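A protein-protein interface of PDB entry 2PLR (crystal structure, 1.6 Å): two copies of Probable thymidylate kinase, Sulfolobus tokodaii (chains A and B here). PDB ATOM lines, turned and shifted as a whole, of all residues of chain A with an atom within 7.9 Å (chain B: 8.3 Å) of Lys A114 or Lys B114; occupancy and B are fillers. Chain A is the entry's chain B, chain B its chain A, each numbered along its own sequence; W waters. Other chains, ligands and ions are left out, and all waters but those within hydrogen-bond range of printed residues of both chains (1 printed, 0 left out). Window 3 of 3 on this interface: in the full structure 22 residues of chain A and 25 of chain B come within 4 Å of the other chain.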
ATOM      1  N   TYR A  99      31.637  10.304  11.227  1.00  0.00           N
ATOM      2  CA  TYR A  99      30.840  10.230  10.002  1.00  0.00           C
ATOM      3  C   TYR A  99      30.124   8.887   9.926  1.00  0.00           C
ATOM      4  O   TYR A  99      28.935   8.816   9.611  1.00  0.00           O
ATOM      5  CB  TYR A  99      31.713  10.349   8.746  1.00  0.00           C
ATOM      6  CG  TYR A  99      32.308  11.711   8.435  1.00  0.00           C
ATOM      7  CD1 TYR A  99      32.899  11.944   7.195  1.00  0.00           C
ATOM      8  CD2 TYR A  99      32.296  12.750   9.364  1.00  0.00           C
ATOM      9  CE1 TYR A  99      33.466  13.170   6.879  1.00  0.00           C
ATOM     10  CE2 TYR A  99      32.869  13.994   9.058  1.00  0.00           C
ATOM     11  CZ  TYR A  99      33.451  14.192   7.811  1.00  0.00           C
ATOM     12  OH  TYR A  99      34.031  15.397   7.482  1.00  0.00           O
ATOM     13  N   ASP A 108      22.104  12.679   9.077  1.00  0.00           N
ATOM     14  CA  ASP A 108      22.554  13.113   7.751  1.00  0.00           C
ATOM     15  C   ASP A 108      24.061  13.330   7.773  1.00  0.00           C
ATOM     16  O   ASP A 108      24.555  14.193   8.497  1.00  0.00           O
ATOM     17  CB  ASP A 108      21.858  14.418   7.356  1.00  0.00           C
ATOM     18  CG  ASP A 108      22.183  14.850   5.930  1.00  0.00           C
ATOM     19  OD1 ASP A 108      23.086  14.255   5.303  1.00  0.00           O
ATOM     20  OD2 ASP A 108      21.534  15.794   5.438  1.00  0.00           O
ATOM     21  N   ILE A 109      24.792  12.558   6.975  1.00  0.00           N
ATOM     22  CA  ILE A 109      26.243  12.674   6.952  1.00  0.00           C
ATOM     23  C   ILE A 109      26.717  14.058   6.522  1.00  0.00           C
ATOM     24  O   ILE A 109      27.785  14.506   6.925  1.00  0.00           O
ATOM     25  CB  ILE A 109      26.878  11.603   6.037  1.00  0.00           C
ATOM     26  CG1 ILE A 109      28.371  11.484   6.348  1.00  0.00           C
ATOM     27  CG2 ILE A 109      26.674  11.974   4.573  1.00  0.00           C
ATOM     28  CD1 ILE A 109      29.051  10.314   5.662  1.00  0.00           C
ATOM     29  N   ASP A 110      25.919  14.740   5.710  1.00  0.00           N
ATOM     30  CA  ASP A 110      26.294  16.070   5.257  1.00  0.00           C
ATOM     31  C   ASP A 110      26.230  17.065   6.410  1.00  0.00           C
ATOM     32  O   ASP A 110      27.006  18.022   6.465  1.00  0.00           O
ATOM     33  CB  ASP A 110      25.386  16.511   4.114  1.00  0.00           C
ATOM     34  CG  ASP A 110      25.650  15.736   2.834  1.00  0.00           C
ATOM     35  OD1 ASP A 110      26.828  15.391   2.577  1.00  0.00           O
ATOM     36  OD2 ASP A 110      24.690  15.492   2.079  1.00  0.00           O
ATOM     37  N   TRP A 111      25.302  16.835   7.333  1.00  0.00           N
ATOM     38  CA  TRP A 111      25.187  17.700   8.499  1.00  0.00           C
ATOM     39  C   TRP A 111      26.380  17.399   9.406  1.00  0.00           C
ATOM     40  O   TRP A 111      26.964  18.306  10.000  1.00  0.00           O
ATOM     41  CB  TRP A 111      23.880  17.422   9.249  1.00  0.00           C
ATOM     42  CG  TRP A 111      23.717  18.240  10.502  1.00  0.00           C
ATOM     43  CD1 TRP A 111      23.319  19.546  10.589  1.00  0.00           C
ATOM     44  CD2 TRP A 111      23.956  17.806  11.845  1.00  0.00           C
ATOM     45  NE1 TRP A 111      23.291  19.947  11.906  1.00  0.00           N
ATOM     46  CE2 TRP A 111      23.682  18.898  12.697  1.00  0.00           C
ATOM     47  CE3 TRP A 111      24.384  16.594  12.412  1.00  0.00           C
ATOM     48  CZ2 TRP A 111      23.814  18.819  14.087  1.00  0.00           C
ATOM     49  CZ3 TRP A 111      24.516  16.516  13.795  1.00  0.00           C
ATOM     50  CH2 TRP A 111      24.234  17.623  14.617  1.00  0.00           C
ATOM     51  N   VAL A 112      26.742  16.120   9.507  1.00  0.00           N
ATOM     52  CA  VAL A 112      27.875  15.729  10.342  1.00  0.00           C
ATOM     53  C   VAL A 112      29.165  16.335   9.790  1.00  0.00           C
ATOM     54  O   VAL A 112      30.045  16.731  10.551  1.00  0.00           O
ATOM     55  CB  VAL A 112      28.017  14.185  10.440  1.00  0.00           C
ATOM     56  CG1 VAL A 112      29.233  13.822  11.292  1.00  0.00           C
ATOM     57  CG2 VAL A 112      26.761  13.587  11.071  1.00  0.00           C
ATOM     58  N   LYS A 113      29.279  16.418   8.467  1.00  0.00           N
ATOM     59  CA  LYS A 113      30.471  17.008   7.866  1.00  0.00           C
ATOM     60  C   LYS A 113      30.542  18.485   8.250  1.00  0.00           C
ATOM     61  O   LYS A 113      31.612  19.003   8.561  1.00  0.00           O
ATOM     62  CB  LYS A 113      30.441  16.854   6.342  1.00  0.00           C
ATOM     63  CG  LYS A 113      30.653  15.417   5.878  1.00  0.00           C
ATOM     64  CD  LYS A 113      30.620  15.305   4.358  1.00  0.00           C
ATOM     65  CE  LYS A 113      30.917  13.879   3.913  1.00  0.00           C
ATOM     66  NZ  LYS A 113      30.913  13.739   2.423  1.00  0.00           N
ATOM     67  N   LYS A 114      29.398  19.161   8.232  1.00  0.00           N
ATOM     68  CA  LYS A 114      29.362  20.570   8.613  1.00  0.00           C
ATOM     69  C   LYS A 114      29.669  20.722  10.102  1.00  0.00           C
ATOM     70  O   LYS A 114      30.359  21.653  10.515  1.00  0.00           O
ATOM     71  CB  LYS A 114      27.989  21.171   8.305  1.00  0.00           C
ATOM     72  CG  LYS A 114      27.693  21.351   6.820  1.00  0.00           C
ATOM     73  CD  LYS A 114      28.568  22.436   6.212  1.00  0.00           C
ATOM     74  CE  LYS A 114      28.134  22.764   4.794  1.00  0.00           C
ATOM     75  NZ  LYS A 114      28.892  23.926   4.257  1.00  0.00           N
ATOM     76  N   LEU A 115      29.156  19.796  10.905  1.00  0.00           N
ATOM     77  CA  LEU A 115      29.368  19.828  12.349  1.00  0.00           C
ATOM     78  C   LEU A 115      30.854  19.804  12.698  1.00  0.00           C
ATOM     79  O   LEU A 115      31.325  20.569  13.545  1.00  0.00           O
ATOM     80  CB  LEU A 115      28.667  18.629  12.997  1.00  0.00           C
ATOM     81  CG  LEU A 115      28.780  18.438  14.511  1.00  0.00           C
ATOM     82  CD1 LEU A 115      28.096  19.586  15.240  1.00  0.00           C
ATOM     83  CD2 LEU A 115      28.142  17.104  14.893  1.00  0.00           C
ATOM     84  N   TYR A 116      31.595  18.929  12.025  1.00  0.00           N
ATOM     85  CA  TYR A 116      33.021  18.788  12.275  1.00  0.00           C
ATOM     86  C   TYR A 116      33.905  19.658  11.384  1.00  0.00           C
ATOM     87  O   TYR A 116      35.127  19.506  11.390  1.00  0.00           O
ATOM     88  CB  TYR A 116      33.432  17.319  12.104  1.00  0.00           C
ATOM     89  CG  TYR A 116      33.019  16.420  13.248  1.00  0.00           C
ATOM     90  CD1 TYR A 116      31.751  15.836  13.294  1.00  0.00           C
ATOM     91  CD2 TYR A 116      33.899  16.162  14.293  1.00  0.00           C
ATOM     92  CE1 TYR A 116      31.375  15.012  14.360  1.00  0.00           C
ATOM     93  CE2 TYR A 116      33.538  15.350  15.358  1.00  0.00           C
ATOM     94  CZ  TYR A 116      32.277  14.776  15.389  1.00  0.00           C
ATOM     95  OH  TYR A 116      31.936  13.969  16.449  1.00  0.00           O
ATOM     96  N   SER A 117      33.299  20.576  10.634  1.00  0.00           N
ATOM     97  CA  SER A 117      34.064  21.430   9.727  1.00  0.00           C
ATOM     98  C   SER A 117      35.049  22.381  10.403  1.00  0.00           C
ATOM     99  O   SER A 117      35.794  23.085   9.718  1.00  0.00           O
ATOM    100  CB  SER A 117      33.124  22.222   8.807  1.00  0.00           C
ATOM    101  OG  SER A 117      32.312  23.133   9.529  1.00  0.00           O
ATOM    102  N   PHE A 118      35.061  22.416  11.732  1.00  0.00           N
ATOM    103  CA  PHE A 118      36.011  23.277  12.429  1.00  0.00           C
ATOM    104  C   PHE A 118      37.368  22.583  12.491  1.00  0.00           C
ATOM    105  O   PHE A 118      38.376  23.205  12.817  1.00  0.00           O
ATOM    106  CB  PHE A 118      35.546  23.593  13.855  1.00  0.00           C
ATOM    107  CG  PHE A 118      35.275  22.377  14.699  1.00  0.00           C
ATOM    108  CD1 PHE A 118      33.980  21.885  14.833  1.00  0.00           C
ATOM    109  CD2 PHE A 118      36.312  21.729  15.368  1.00  0.00           C
ATOM    110  CE1 PHE A 118      33.715  20.768  15.623  1.00  0.00           C
ATOM    111  CE2 PHE A 118      36.059  20.606  16.163  1.00  0.00           C
ATOM    112  CZ  PHE A 118      34.755  20.124  16.292  1.00  0.00           C
ATOM    113  N   ALA A 119      37.384  21.293  12.168  1.00  0.00           N
ATOM    114  CA  ALA A 119      38.608  20.502  12.203  1.00  0.00           C
ATOM    115  C   ALA A 119      39.242  20.343  10.825  1.00  0.00           C
ATOM    116  O   ALA A 119      38.550  20.160   9.827  1.00  0.00           O
ATOM    117  CB  ALA A 119      38.316  19.128  12.798  1.00  0.00           C
ATOM    118  N   TYR B  99      22.759  31.689  19.315  1.00  0.00           N
ATOM    119  CA  TYR B  99      23.399  32.340  18.169  1.00  0.00           C
ATOM    120  C   TYR B  99      24.200  33.534  18.691  1.00  0.00           C
ATOM    121  O   TYR B  99      25.356  33.740  18.322  1.00  0.00           O
ATOM    122  CB  TYR B  99      22.375  32.911  17.179  1.00  0.00           C
ATOM    123  CG  TYR B  99      21.634  31.956  16.259  1.00  0.00           C
ATOM    124  CD1 TYR B  99      20.946  32.459  15.154  1.00  0.00           C
ATOM    125  CD2 TYR B  99      21.575  30.581  16.505  1.00  0.00           C
ATOM    126  CE1 TYR B  99      20.214  31.628  14.314  1.00  0.00           C
ATOM    127  CE2 TYR B  99      20.832  29.731  15.661  1.00  0.00           C
ATOM    128  CZ  TYR B  99      20.157  30.269  14.572  1.00  0.00           C
ATOM    129  OH  TYR B  99      19.396  29.468  13.742  1.00  0.00           O
ATOM    130  N   ASP B 108      31.714  30.828  14.720  1.00  0.00           N
ATOM    131  CA  ASP B 108      31.166  31.237  13.430  1.00  0.00           C
ATOM    132  C   ASP B 108      29.643  31.172  13.386  1.00  0.00           C
ATOM    133  O   ASP B 108      29.044  30.136  13.661  1.00  0.00           O
ATOM    134  CB  ASP B 108      31.766  30.378  12.312  1.00  0.00           C
ATOM    135  CG  ASP B 108      31.271  30.781  10.938  1.00  0.00           C
ATOM    136  OD1 ASP B 108      30.220  30.265  10.503  1.00  0.00           O
ATOM    137  OD2 ASP B 108      31.935  31.623  10.296  1.00  0.00           O
ATOM    138  N   ILE B 109      29.026  32.293  13.019  1.00  0.00           N
ATOM    139  CA  ILE B 109      27.572  32.392  12.964  1.00  0.00           C
ATOM    140  C   ILE B 109      26.905  31.394  12.019  1.00  0.00           C
ATOM    141  O   ILE B 109      25.861  30.830  12.354  1.00  0.00           O
ATOM    142  CB  ILE B 109      27.122  33.835  12.585  1.00  0.00           C
ATOM    143  CG1 ILE B 109      25.601  33.957  12.706  1.00  0.00           C
ATOM    144  CG2 ILE B 109      27.574  34.179  11.174  1.00  0.00           C
ATOM    145  CD1 ILE B 109      25.075  33.737  14.119  1.00  0.00           C
ATOM    146  N   ASP B 110      27.494  31.178  10.846  1.00  0.00           N
ATOM    147  CA  ASP B 110      26.918  30.237   9.890  1.00  0.00           C
ATOM    148  C   ASP B 110      26.980  28.812  10.441  1.00  0.00           C
ATOM    149  O   ASP B 110      26.058  28.017  10.241  1.00  0.00           O
ATOM    150  CB  ASP B 110      27.652  30.311   8.546  1.00  0.00           C
ATOM    151  CG  ASP B 110      27.428  31.635   7.832  1.00  0.00           C
ATOM    152  OD1 ASP B 110      26.272  32.099   7.796  1.00  0.00           O
ATOM    153  OD2 ASP B 110      28.405  32.204   7.299  1.00  0.00           O
ATOM    154  N   TRP B 111      28.064  28.500  11.142  1.00  0.00           N
ATOM    155  CA  TRP B 111      28.235  27.175  11.725  1.00  0.00           C
ATOM    156  C   TRP B 111      27.193  26.928  12.822  1.00  0.00           C
ATOM    157  O   TRP B 111      26.608  25.848  12.898  1.00  0.00           O
ATOM    158  CB  TRP B 111      29.648  27.030  12.299  1.00  0.00           C
ATOM    159  CG  TRP B 111      29.935  25.673  12.875  1.00  0.00           C
ATOM    160  CD1 TRP B 111      30.376  24.565  12.204  1.00  0.00           C
ATOM    161  CD2 TRP B 111      29.790  25.282  14.242  1.00  0.00           C
ATOM    162  NE1 TRP B 111      30.518  23.509  13.072  1.00  0.00           N
ATOM    163  CE2 TRP B 111      30.165  23.922  14.331  1.00  0.00           C
ATOM    164  CE3 TRP B 111      29.382  25.952  15.406  1.00  0.00           C
ATOM    165  CZ2 TRP B 111      30.139  23.216  15.540  1.00  0.00           C
ATOM    166  CZ3 TRP B 111      29.357  25.251  16.606  1.00  0.00           C
ATOM    167  CH2 TRP B 111      29.736  23.896  16.663  1.00  0.00           C
ATOM    168  N   VAL B 112      26.952  27.928  13.667  1.00  0.00           N
ATOM    169  CA  VAL B 112      25.973  27.775  14.737  1.00  0.00           C
ATOM    170  C   VAL B 112      24.558  27.623  14.174  1.00  0.00           C
ATOM    171  O   VAL B 112      23.739  26.885  14.718  1.00  0.00           O
ATOM    172  CB  VAL B 112      26.010  28.976  15.714  1.00  0.00           C
ATOM    173  CG1 VAL B 112      24.995  28.772  16.833  1.00  0.00           C
ATOM    174  CG2 VAL B 112      27.404  29.126  16.296  1.00  0.00           C
ATOM    175  N   LYS B 113      24.260  28.319  13.082  1.00  0.00           N
ATOM    176  CA  LYS B 113      22.936  28.191  12.489  1.00  0.00           C
ATOM    177  C   LYS B 113      22.755  26.772  11.965  1.00  0.00           C
ATOM    178  O   LYS B 113      21.692  26.180  12.129  1.00  0.00           O
ATOM    179  CB  LYS B 113      22.753  29.192  11.353  1.00  0.00           C
ATOM    180  CG  LYS B 113      22.619  30.635  11.815  1.00  0.00           C
ATOM    181  CD  LYS B 113      22.485  31.537  10.606  1.00  0.00           C
ATOM    182  CE  LYS B 113      22.303  32.984  10.977  1.00  0.00           C
ATOM    183  NZ  LYS B 113      22.306  33.806   9.731  1.00  0.00           N
ATOM    184  N   LYS B 114      23.796  26.223  11.345  1.00  0.00           N
ATOM    185  CA  LYS B 114      23.719  24.863  10.819  1.00  0.00           C
ATOM    186  C   LYS B 114      23.596  23.866  11.972  1.00  0.00           C
ATOM    187  O   LYS B 114      22.859  22.884  11.885  1.00  0.00           O
ATOM    188  CB  LYS B 114      24.960  24.546   9.976  1.00  0.00           C
ATOM    189  CG  LYS B 114      24.966  23.143   9.379  1.00  0.00           C
ATOM    190  CD  LYS B 114      23.856  22.942   8.354  1.00  0.00           C
ATOM    191  CE  LYS B 114      24.079  23.786   7.107  1.00  0.00           C
ATOM    192  NZ  LYS B 114      23.129  23.409   6.015  1.00  0.00           N
ATOM    193  N   LEU B 115      24.317  24.129  13.058  1.00  0.00           N
ATOM    194  CA  LEU B 115      24.285  23.264  14.232  1.00  0.00           C
ATOM    195  C   LEU B 115      22.863  23.089  14.762  1.00  0.00           C
ATOM    196  O   LEU B 115      22.437  21.982  15.083  1.00  0.00           O
ATOM    197  CB  LEU B 115      25.175  23.856  15.331  1.00  0.00           C
ATOM    198  CG  LEU B 115      25.126  23.254  16.737  1.00  0.00           C
ATOM    199  CD1 LEU B 115      25.724  21.848  16.734  1.00  0.00           C
ATOM    200  CD2 LEU B 115      25.905  24.155  17.689  1.00  0.00           C
ATOM    201  N   TYR B 116      22.127  24.193  14.838  1.00  0.00           N
ATOM    202  CA  TYR B 116      20.767  24.166  15.357  1.00  0.00           C
ATOM    203  C   TYR B 116      19.684  23.926  14.312  1.00  0.00           C
ATOM    204  O   TYR B 116      18.491  24.039  14.615  1.00  0.00           O
ATOM    205  CB  TYR B 116      20.485  25.476  16.096  1.00  0.00           C
ATOM    206  CG  TYR B 116      21.076  25.520  17.484  1.00  0.00           C
ATOM    207  CD1 TYR B 116      20.435  24.894  18.552  1.00  0.00           C
ATOM    208  CD2 TYR B 116      22.282  26.178  17.731  1.00  0.00           C
ATOM    209  CE1 TYR B 116      20.978  24.913  19.833  1.00  0.00           C
ATOM    210  CE2 TYR B 116      22.836  26.204  19.011  1.00  0.00           C
ATOM    211  CZ  TYR B 116      22.176  25.573  20.056  1.00  0.00           C
ATOM    212  OH  TYR B 116      22.698  25.592  21.322  1.00  0.00           O
ATOM    213  N   SER B 117      20.085  23.581  13.093  1.00  0.00           N
ATOM    214  CA  SER B 117      19.112  23.355  12.029  1.00  0.00           C
ATOM    215  C   SER B 117      18.184  22.168  12.286  1.00  0.00           C
ATOM    216  O   SER B 117      17.237  21.953  11.537  1.00  0.00           O
ATOM    217  CB  SER B 117      19.821  23.193  10.680  1.00  0.00           C
ATOM    218  OG  SER B 117      20.683  22.070  10.674  1.00  0.00           O
ATOM    219  N   PHE B 118      18.442  21.403  13.342  1.00  0.00           N
ATOM    220  CA  PHE B 118      17.581  20.267  13.663  1.00  0.00           C
ATOM    221  C   PHE B 118      16.318  20.742  14.377  1.00  0.00           C
ATOM    222  O   PHE B 118      15.346  19.996  14.503  1.00  0.00           O
ATOM    223  CB  PHE B 118      18.311  19.262  14.560  1.00  0.00           C
ATOM    224  CG  PHE B 118      18.725  19.823  15.892  1.00  0.00           C
ATOM    225  CD1 PHE B 118      20.013  20.314  16.086  1.00  0.00           C
ATOM    226  CD2 PHE B 118      17.821  19.873  16.951  1.00  0.00           C
ATOM    227  CE1 PHE B 118      20.396  20.844  17.317  1.00  0.00           C
ATOM    228  CE2 PHE B 118      18.193  20.402  18.183  1.00  0.00           C
ATOM    229  CZ  PHE B 118      19.488  20.889  18.366  1.00  0.00           C
ATOM    230  N   ALA B 119      16.340  21.985  14.846  1.00  0.00           N
ATOM    231  CA  ALA B 119      15.209  22.557  15.571  1.00  0.00           C
ATOM    232  C   ALA B 119      14.315  23.409  14.685  1.00  0.00           C
ATOM    233  O   ALA B 119      14.794  24.157  13.835  1.00  0.00           O
ATOM    234  CB  ALA B 119      15.714  23.388  16.748  1.00  0.00           C
HETATM  235  O   HOH W   1      27.638  23.358  11.521  1.00  0.00           O
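The backbone carbonyl oxygen of Lys A114 lies within hydrogen-bond range of the indole nitrogen of Trp B111 (3.2 Å).
NE1 of Trp A111 lies within hydrogen-bond range of O of Lys B114 (3.0 Å).
NE1 of Trp B111 lies within hydrogen-bond range of O of Leu A115 (3.1 Å).
O of Lys B114 is in hydrogen-bond range of OG of Ser B117, 2.6 Å away.
The backbone carbonyl oxygen of Lys A114 sits at hydrogen-bond distance from the side-chain hydroxyl of Ser A117 (2.6 Å).
The side-chain carboxylate of Asp B108 is in hydrogen-bond range of the backbone NH of Trp B111 (2.9 Å).
O of Leu B115 touches CZ2 of Trp A111 (3.6 Å).
Ser B117 touches Trp A111 (OG to NE1, 3.6 Å).
CG of Lys B114 touches CB of Lys A114 (3.8 Å).
Leu A115 touches Leu B115.
Trp B111 touches Ser A117.
Of the printed residues of chain B, Trp A111 touches Lys B114 (3.0 Å), Leu B115 (3.6 Å) and Ser B117 (3.6 Å).
Lys A114 touches just these residues of chain B: Trp B111 and Lys B114.
Of the printed residues of chain A, Trp B111 touches Lys A114, Leu A115 and Ser A117.
Lys B114 touches two residues of chain A.
Of the printed residues of chain A, Leu B115 touches Trp A111 and Leu A115.
Printed residues of chain A within 4 Å of Ser B117: Trp A111.
The nearest residue of chain A that does not touch Lys B114 is Leu A115 (5.6 Å).
The nearest printed residue of chain A that does not touch Trp B111 is Phe A118 (4.1 Å).
Hydrophobic or aromatic side chains of chain A that line the printed part of chain B: Trp A111 and Leu A115.
Hydrophobic or aromatic side chains of chain B within 4 Å of the printed part of chain A: Trp B111 and Leu B115.
Among the printed residues, no Asp or Glu carboxylate lies within 4 Å of a Lys or Arg side-chain nitrogen of the other chain.
Trp A111 touches Lys B114, and with the chains exchanged Lys A114 touches Trp B111.
Trp A111 touches Leu B115, and with the chains exchanged Leu A115 touches Trp B111.
Trp A111 touches Ser B117, and with the chains exchanged Ser A117 touches Trp B111.
Leu A115 touches its own counterpart, Leu B115.
Of the 8 pairs that touch across the chains among the printed residues, 8 have their exchanged pair printed and touching as well.
Water W1 lies within hydrogen-bond range of O of Trp B111 and O of Lys A114.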
